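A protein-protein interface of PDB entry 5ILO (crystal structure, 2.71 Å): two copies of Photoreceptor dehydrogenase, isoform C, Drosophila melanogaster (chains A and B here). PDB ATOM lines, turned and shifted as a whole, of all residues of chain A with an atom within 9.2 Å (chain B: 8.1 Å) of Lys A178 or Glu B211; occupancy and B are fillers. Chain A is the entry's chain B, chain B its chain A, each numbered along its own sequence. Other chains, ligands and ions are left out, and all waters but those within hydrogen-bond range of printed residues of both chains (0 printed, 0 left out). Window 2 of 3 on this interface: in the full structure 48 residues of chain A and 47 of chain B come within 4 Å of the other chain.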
ATOM      1  N   ASP A 134      -4.680  -5.853  -9.285  1.00  0.00           N
ATOM      2  CA  ASP A 134      -4.716  -4.403  -9.472  1.00  0.00           C
ATOM      3  C   ASP A 134      -5.954  -3.903 -10.224  1.00  0.00           C
ATOM      4  O   ASP A 134      -6.330  -2.736 -10.098  1.00  0.00           O
ATOM      5  CB  ASP A 134      -3.452  -3.941 -10.208  1.00  0.00           C
ATOM      6  CG  ASP A 134      -3.225  -4.689 -11.511  1.00  0.00           C
ATOM      7  OD1 ASP A 134      -3.639  -5.863 -11.610  1.00  0.00           O
ATOM      8  OD2 ASP A 134      -2.635  -4.099 -12.440  1.00  0.00           O
ATOM      9  N   ASN A 135      -6.588  -4.781 -10.998  1.00  0.00           N
ATOM     10  CA  ASN A 135      -7.853  -4.446 -11.650  1.00  0.00           C
ATOM     11  C   ASN A 135      -9.068  -5.025 -10.931  1.00  0.00           C
ATOM     12  O   ASN A 135     -10.130  -5.197 -11.534  1.00  0.00           O
ATOM     13  CB  ASN A 135      -7.842  -4.910 -13.109  1.00  0.00           C
ATOM     14  CG  ASN A 135      -7.395  -3.818 -14.066  1.00  0.00           C
ATOM     15  OD1 ASN A 135      -6.748  -2.849 -13.663  1.00  0.00           O
ATOM     16  ND2 ASN A 135      -7.742  -3.966 -15.339  1.00  0.00           N
ATOM     17  N   CYS A 173       8.617 -15.292 -19.576  1.00  0.00           N
ATOM     18  CA  CYS A 173       8.740 -13.848 -19.361  1.00  0.00           C
ATOM     19  C   CYS A 173       7.746 -13.325 -18.340  1.00  0.00           C
ATOM     20  O   CYS A 173       8.117 -12.635 -17.389  1.00  0.00           O
ATOM     21  CB  CYS A 173       8.538 -13.081 -20.671  1.00  0.00           C
ATOM     22  SG  CYS A 173       9.977 -13.008 -21.743  1.00  0.00           S
ATOM     23  N   LEU A 174       6.475 -13.645 -18.562  1.00  0.00           N
ATOM     24  CA  LEU A 174       5.388 -13.139 -17.735  1.00  0.00           C
ATOM     25  C   LEU A 174       5.452 -13.659 -16.297  1.00  0.00           C
ATOM     26  O   LEU A 174       4.790 -13.126 -15.409  1.00  0.00           O
ATOM     27  CB  LEU A 174       4.039 -13.483 -18.379  1.00  0.00           C
ATOM     28  CG  LEU A 174       3.795 -12.880 -19.771  1.00  0.00           C
ATOM     29  CD1 LEU A 174       2.366 -13.100 -20.228  1.00  0.00           C
ATOM     30  CD2 LEU A 174       4.139 -11.394 -19.800  1.00  0.00           C
ATOM     31  N   ALA A 175       6.263 -14.690 -16.071  1.00  0.00           N
ATOM     32  CA  ALA A 175       6.439 -15.275 -14.740  1.00  0.00           C
ATOM     33  C   ALA A 175       7.388 -14.472 -13.849  1.00  0.00           C
ATOM     34  O   ALA A 175       8.061 -15.031 -12.983  1.00  0.00           O
ATOM     35  CB  ALA A 175       6.933 -16.706 -14.863  1.00  0.00           C
ATOM     36  N   ASN A 176       7.418 -13.159 -14.054  1.00  0.00           N
ATOM     37  CA  ASN A 176       8.280 -12.262 -13.288  1.00  0.00           C
ATOM     38  C   ASN A 176       7.781 -12.032 -11.864  1.00  0.00           C
ATOM     39  O   ASN A 176       6.584 -11.856 -11.644  1.00  0.00           O
ATOM     40  CB  ASN A 176       8.397 -10.917 -14.009  1.00  0.00           C
ATOM     41  CG  ASN A 176       9.419 -10.004 -13.373  1.00  0.00           C
ATOM     42  OD1 ASN A 176       9.096  -8.892 -12.955  1.00  0.00           O
ATOM     43  ND2 ASN A 176      10.659 -10.468 -13.290  1.00  0.00           N
ATOM     44  N   GLU A 177       8.703 -12.036 -10.902  1.00  0.00           N
ATOM     45  CA  GLU A 177       8.344 -11.851  -9.498  1.00  0.00           C
ATOM     46  C   GLU A 177       7.663 -10.515  -9.238  1.00  0.00           C
ATOM     47  O   GLU A 177       6.695 -10.442  -8.481  1.00  0.00           O
ATOM     48  CB  GLU A 177       9.577 -11.955  -8.600  1.00  0.00           C
ATOM     49  CG  GLU A 177      10.171 -13.342  -8.476  1.00  0.00           C
ATOM     50  CD  GLU A 177      11.259 -13.396  -7.420  1.00  0.00           C
ATOM     51  OE1 GLU A 177      11.657 -12.320  -6.924  1.00  0.00           O
ATOM     52  OE2 GLU A 177      11.714 -14.510  -7.081  1.00  0.00           O
ATOM     53  N   LYS A 178       8.180  -9.461  -9.863  1.00  0.00           N
ATOM     54  CA  LYS A 178       7.608  -8.127  -9.719  1.00  0.00           C
ATOM     55  C   LYS A 178       6.188  -8.061 -10.271  1.00  0.00           C
ATOM     56  O   LYS A 178       5.319  -7.423  -9.676  1.00  0.00           O
ATOM     57  CB  LYS A 178       8.487  -7.082 -10.412  1.00  0.00           C
ATOM     58  CG  LYS A 178       7.951  -5.658 -10.304  1.00  0.00           C
ATOM     59  CD  LYS A 178       8.785  -4.674 -11.110  1.00  0.00           C
ATOM     60  CE  LYS A 178       8.221  -3.263 -11.003  1.00  0.00           C
ATOM     61  NZ  LYS A 178       8.974  -2.286 -11.840  1.00  0.00           N
ATOM     62  N   TYR A 179       5.957  -8.708 -11.411  1.00  0.00           N
ATOM     63  CA  TYR A 179       4.622  -8.731 -11.997  1.00  0.00           C
ATOM     64  C   TYR A 179       3.643  -9.514 -11.131  1.00  0.00           C
ATOM     65  O   TYR A 179       2.491  -9.114 -10.971  1.00  0.00           O
ATOM     66  CB  TYR A 179       4.635  -9.311 -13.411  1.00  0.00           C
ATOM     67  CG  TYR A 179       3.295  -9.139 -14.093  1.00  0.00           C
ATOM     68  CD1 TYR A 179       2.750  -7.873 -14.273  1.00  0.00           C
ATOM     69  CD2 TYR A 179       2.566 -10.235 -14.538  1.00  0.00           C
ATOM     70  CE1 TYR A 179       1.523  -7.700 -14.884  1.00  0.00           C
ATOM     71  CE2 TYR A 179       1.335 -10.072 -15.153  1.00  0.00           C
ATOM     72  CZ  TYR A 179       0.819  -8.800 -15.322  1.00  0.00           C
ATOM     73  OH  TYR A 179      -0.403  -8.622 -15.933  1.00  0.00           O
ATOM     74  N   TYR A 180       4.105 -10.631 -10.579  1.00  0.00           N
ATOM     75  CA  TYR A 180       3.244 -11.484  -9.765  1.00  0.00           C
ATOM     76  C   TYR A 180       2.801 -10.777  -8.493  1.00  0.00           C
ATOM     77  O   TYR A 180       1.639 -10.861  -8.097  1.00  0.00           O
ATOM     78  CB  TYR A 180       3.948 -12.789  -9.396  1.00  0.00           C
ATOM     79  CG  TYR A 180       3.175 -13.596  -8.376  1.00  0.00           C
ATOM     80  CD1 TYR A 180       1.917 -14.112  -8.673  1.00  0.00           C
ATOM     81  CD2 TYR A 180       3.685 -13.804  -7.100  1.00  0.00           C
ATOM     82  CE1 TYR A 180       1.202 -14.836  -7.733  1.00  0.00           C
ATOM     83  CE2 TYR A 180       2.979 -14.525  -6.156  1.00  0.00           C
ATOM     84  CZ  TYR A 180       1.741 -15.039  -6.475  1.00  0.00           C
ATOM     85  OH  TYR A 180       1.042 -15.754  -5.533  1.00  0.00           O
ATOM     86  N   GLN A 181       3.736 -10.085  -7.851  1.00  0.00           N
ATOM     87  CA  GLN A 181       3.429  -9.332  -6.643  1.00  0.00           C
ATOM     88  C   GLN A 181       2.412  -8.222  -6.920  1.00  0.00           C
ATOM     89  O   GLN A 181       1.611  -7.866  -6.056  1.00  0.00           O
ATOM     90  CB  GLN A 181       4.709  -8.732  -6.055  1.00  0.00           C
ATOM     91  CG  GLN A 181       5.541  -9.696  -5.204  1.00  0.00           C
ATOM     92  CD  GLN A 181       4.776 -10.341  -4.057  1.00  0.00           C
ATOM     93  OE1 GLN A 181       3.718  -9.866  -3.639  1.00  0.00           O
ATOM     94  NE2 GLN A 181       5.320 -11.437  -3.539  1.00  0.00           N
ATOM     95  N   ARG A 182       2.453  -7.677  -8.130  1.00  0.00           N
ATOM     96  CA  ARG A 182       1.512  -6.643  -8.543  1.00  0.00           C
ATOM     97  C   ARG A 182       0.173  -7.195  -9.031  1.00  0.00           C
ATOM     98  O   ARG A 182      -0.887  -6.674  -8.683  1.00  0.00           O
ATOM     99  CB  ARG A 182       2.147  -5.779  -9.634  1.00  0.00           C
ATOM    100  CG  ARG A 182       1.210  -4.772 -10.280  1.00  0.00           C
ATOM    101  CD  ARG A 182       1.851  -4.140 -11.517  1.00  0.00           C
ATOM    102  NE  ARG A 182       3.297  -4.362 -11.549  1.00  0.00           N
ATOM    103  CZ  ARG A 182       4.027  -4.525 -12.649  1.00  0.00           C
ATOM    104  NH1 ARG A 182       3.470  -4.456 -13.849  1.00  0.00           N
ATOM    105  NH2 ARG A 182       5.335  -4.723 -12.541  1.00  0.00           N
ATOM    106  N   SER A 183       0.228  -8.258  -9.829  1.00  0.00           N
ATOM    107  CA  SER A 183      -0.957  -8.771 -10.513  1.00  0.00           C
ATOM    108  C   SER A 183      -1.587  -9.958  -9.791  1.00  0.00           C
ATOM    109  O   SER A 183      -2.810 -10.077  -9.737  1.00  0.00           O
ATOM    110  CB  SER A 183      -0.607  -9.164 -11.953  1.00  0.00           C
ATOM    111  OG  SER A 183       0.164 -10.354 -11.986  1.00  0.00           O
ATOM    112  N   GLY A 184      -0.751 -10.836  -9.247  1.00  0.00           N
ATOM    113  CA  GLY A 184      -1.231 -12.048  -8.606  1.00  0.00           C
ATOM    114  C   GLY A 184      -1.464 -13.197  -9.568  1.00  0.00           C
ATOM    115  O   GLY A 184      -1.892 -14.278  -9.161  1.00  0.00           O
ATOM    116  N   ILE A 185      -1.184 -12.963 -10.847  1.00  0.00           N
ATOM    117  CA  ILE A 185      -1.353 -13.978 -11.883  1.00  0.00           C
ATOM    118  C   ILE A 185      -0.084 -14.811 -12.035  1.00  0.00           C
ATOM    119  O   ILE A 185       1.014 -14.259 -12.109  1.00  0.00           O
ATOM    120  CB  ILE A 185      -1.697 -13.337 -13.243  1.00  0.00           C
ATOM    121  CG1 ILE A 185      -2.913 -12.417 -13.110  1.00  0.00           C
ATOM    122  CG2 ILE A 185      -1.915 -14.408 -14.309  1.00  0.00           C
ATOM    123  CD1 ILE A 185      -3.126 -11.519 -14.311  1.00  0.00           C
ATOM    124  N   ASN A 244       4.421 -20.934 -10.091  1.00  0.00           N
ATOM    125  CA  ASN A 244       4.719 -19.896 -11.072  1.00  0.00           C
ATOM    126  C   ASN A 244       6.001 -20.174 -11.840  1.00  0.00           C
ATOM    127  O   ASN A 244       7.010 -20.566 -11.256  1.00  0.00           O
ATOM    128  CB  ASN A 244       4.822 -18.529 -10.389  1.00  0.00           C
ATOM    129  CG  ASN A 244       4.676 -17.372 -11.364  1.00  0.00           C
ATOM    130  OD1 ASN A 244       4.205 -17.544 -12.489  1.00  0.00           O
ATOM    131  ND2 ASN A 244       5.084 -16.183 -10.933  1.00  0.00           N
ATOM    132  N   PHE B 155      11.788 -10.306 -19.376  1.00  0.00           N
ATOM    133  CA  PHE B 155      10.431  -9.986 -18.945  1.00  0.00           C
ATOM    134  C   PHE B 155       9.830  -8.704 -19.534  1.00  0.00           C
ATOM    135  O   PHE B 155       8.613  -8.617 -19.702  1.00  0.00           O
ATOM    136  CB  PHE B 155      10.411  -9.932 -17.411  1.00  0.00           C
ATOM    137  CG  PHE B 155      11.553  -9.146 -16.816  1.00  0.00           C
ATOM    138  CD1 PHE B 155      12.760  -9.776 -16.525  1.00  0.00           C
ATOM    139  CD2 PHE B 155      11.436  -7.791 -16.561  1.00  0.00           C
ATOM    140  CE1 PHE B 155      13.822  -9.072 -15.989  1.00  0.00           C
ATOM    141  CE2 PHE B 155      12.499  -7.079 -16.022  1.00  0.00           C
ATOM    142  CZ  PHE B 155      13.692  -7.722 -15.737  1.00  0.00           C
ATOM    143  N   THR B 204      10.489   2.541 -24.420  1.00  0.00           N
ATOM    144  CA  THR B 204       9.320   2.496 -23.546  1.00  0.00           C
ATOM    145  C   THR B 204       8.005   2.824 -24.252  1.00  0.00           C
ATOM    146  O   THR B 204       6.934   2.626 -23.686  1.00  0.00           O
ATOM    147  CB  THR B 204       9.484   3.465 -22.359  1.00  0.00           C
ATOM    148  OG1 THR B 204       9.579   4.811 -22.844  1.00  0.00           O
ATOM    149  CG2 THR B 204      10.733   3.124 -21.561  1.00  0.00           C
ATOM    150  N   ILE B 207       6.715  -1.056 -25.512  1.00  0.00           N
ATOM    151  CA  ILE B 207       6.587  -2.158 -24.564  1.00  0.00           C
ATOM    152  C   ILE B 207       5.164  -2.262 -24.030  1.00  0.00           C
ATOM    153  O   ILE B 207       4.450  -1.266 -23.939  1.00  0.00           O
ATOM    154  CB  ILE B 207       7.568  -2.011 -23.383  1.00  0.00           C
ATOM    155  CG1 ILE B 207       7.364  -0.671 -22.672  1.00  0.00           C
ATOM    156  CG2 ILE B 207       9.004  -2.154 -23.866  1.00  0.00           C
ATOM    157  CD1 ILE B 207       8.267  -0.475 -21.468  1.00  0.00           C
ATOM    158  N   ILE B 208       4.759  -3.482 -23.688  1.00  0.00           N
ATOM    159  CA  ILE B 208       3.391  -3.760 -23.258  1.00  0.00           C
ATOM    160  C   ILE B 208       3.099  -3.190 -21.870  1.00  0.00           C
ATOM    161  O   ILE B 208       2.175  -2.396 -21.707  1.00  0.00           O
ATOM    162  CB  ILE B 208       3.109  -5.277 -23.258  1.00  0.00           C
ATOM    163  CG1 ILE B 208       3.038  -5.805 -24.692  1.00  0.00           C
ATOM    164  CG2 ILE B 208       1.829  -5.592 -22.491  1.00  0.00           C
ATOM    165  CD1 ILE B 208       3.350  -7.279 -24.812  1.00  0.00           C
ATOM    166  N   PHE B 209       3.884  -3.600 -20.878  1.00  0.00           N
ATOM    167  CA  PHE B 209       3.710  -3.124 -19.507  1.00  0.00           C
ATOM    168  C   PHE B 209       4.481  -1.818 -19.294  1.00  0.00           C
ATOM    169  O   PHE B 209       5.709  -1.827 -19.205  1.00  0.00           O
ATOM    170  CB  PHE B 209       4.176  -4.187 -18.509  1.00  0.00           C
ATOM    171  CG  PHE B 209       3.504  -5.522 -18.685  1.00  0.00           C
ATOM    172  CD1 PHE B 209       2.158  -5.684 -18.399  1.00  0.00           C
ATOM    173  CD2 PHE B 209       4.221  -6.617 -19.143  1.00  0.00           C
ATOM    174  CE1 PHE B 209       1.540  -6.913 -18.564  1.00  0.00           C
ATOM    175  CE2 PHE B 209       3.608  -7.850 -19.310  1.00  0.00           C
ATOM    176  CZ  PHE B 209       2.265  -7.996 -19.020  1.00  0.00           C
ATOM    177  N   PRO B 210       3.759  -0.689 -19.219  1.00  0.00           N
ATOM    178  CA  PRO B 210       4.377   0.643 -19.218  1.00  0.00           C
ATOM    179  C   PRO B 210       5.102   1.053 -17.930  1.00  0.00           C
ATOM    180  O   PRO B 210       6.004   1.888 -17.993  1.00  0.00           O
ATOM    181  CB  PRO B 210       3.183   1.567 -19.463  1.00  0.00           C
ATOM    182  CG  PRO B 210       2.031   0.853 -18.844  1.00  0.00           C
ATOM    183  CD  PRO B 210       2.303  -0.624 -18.991  1.00  0.00           C
ATOM    184  N   GLU B 211       4.723   0.486 -16.790  1.00  0.00           N
ATOM    185  CA  GLU B 211       5.295   0.901 -15.508  1.00  0.00           C
ATOM    186  C   GLU B 211       6.589   0.180 -15.129  1.00  0.00           C
ATOM    187  O   GLU B 211       7.106   0.370 -14.027  1.00  0.00           O
ATOM    188  CB  GLU B 211       4.266   0.718 -14.386  1.00  0.00           C
ATOM    189  CG  GLU B 211       3.761  -0.705 -14.214  1.00  0.00           C
ATOM    190  CD  GLU B 211       2.586  -1.024 -15.118  1.00  0.00           C
ATOM    191  OE1 GLU B 211       1.707  -0.151 -15.282  1.00  0.00           O
ATOM    192  OE2 GLU B 211       2.545  -2.145 -15.666  1.00  0.00           O
ATOM    193  N   THR B 212       7.121  -0.633 -16.033  1.00  0.00           N
ATOM    194  CA  THR B 212       8.313  -1.413 -15.715  1.00  0.00           C
ATOM    195  C   THR B 212       9.631  -0.749 -16.115  1.00  0.00           C
ATOM    196  O   THR B 212       9.859  -0.439 -17.284  1.00  0.00           O
ATOM    197  CB  THR B 212       8.244  -2.803 -16.377  1.00  0.00           C
ATOM    198  OG1 THR B 212       8.074  -2.656 -17.792  1.00  0.00           O
ATOM    199  CG2 THR B 212       7.080  -3.598 -15.808  1.00  0.00           C
ATOM    200  N   SER B 213      10.485  -0.521 -15.118  1.00  0.00           N
ATOM    201  CA  SER B 213      11.833  -0.010 -15.345  1.00  0.00           C
ATOM    202  C   SER B 213      12.687  -1.036 -16.083  1.00  0.00           C
ATOM    203  O   SER B 213      13.049  -2.071 -15.520  1.00  0.00           O
ATOM    204  CB  SER B 213      12.502   0.371 -14.021  1.00  0.00           C
ATOM    205  OG  SER B 213      11.870   1.492 -13.427  1.00  0.00           O
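OE2 of Glu B211 lies within salt-bridge range of NH1 of Arg A182, 3.1 Å away.
The backbone carbonyl oxygen of Phe B209 lies within hydrogen-bond range of the side-chain hydroxyl of Thr B212 (2.9 Å).
The side-chain amide oxygen (OD1) of Asn A176 sits close to the backbone NH (N) of Lys A178 (3.3 Å).
O of Tyr A179 lies within hydrogen-bond range of OG of Ser A183 (2.8 Å).
Among the printed residues, pairs that only touch across the chains: Cys A173 with Phe B155 (3.5 Å), Leu A174 with Phe B209 (3.6 Å), Tyr A179 with Phe B209 (3.7 Å), Asn A176 with Phe B155 (3.9 Å), Arg A182 with Thr B212 (3.9 Å) and Lys A178 with Glu B211 (3.9 Å).
Printed residues of chain B within 4 Å of Lys A178: Glu B211 (3.9 Å).
Of chain A, only Lys A178 and Arg A182 come within 4 Å of Glu B211.
Of the printed residues of chain A, Phe B209 touches Leu A174 and Tyr A179.
Printed residues of chain B within 4 Å of Cys A173: Phe B155 (3.5 Å).
Printed residues of chain B within 4 Å of Leu A174: Phe B209.
Of the printed residues of chain A, Phe B155 touches Cys A173 (3.5 Å) and Asn A176 (3.9 Å).
Of the printed residues of chain B, Tyr A179 touches Phe B209.
The nearest printed residue of chain B that does not touch Lys A178 is Ser B213 (4.02 Å).
Printed residues of chain B that touch a printed residue of chain A: Phe B155, Phe B209, Glu B211 and Thr B212.
Among the printed residues, Asp or Glu carboxylates within 4 Å of a Lys or Arg side-chain nitrogen of the other chain: Arg A182 with Glu B211.
No position is printed for both chains.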
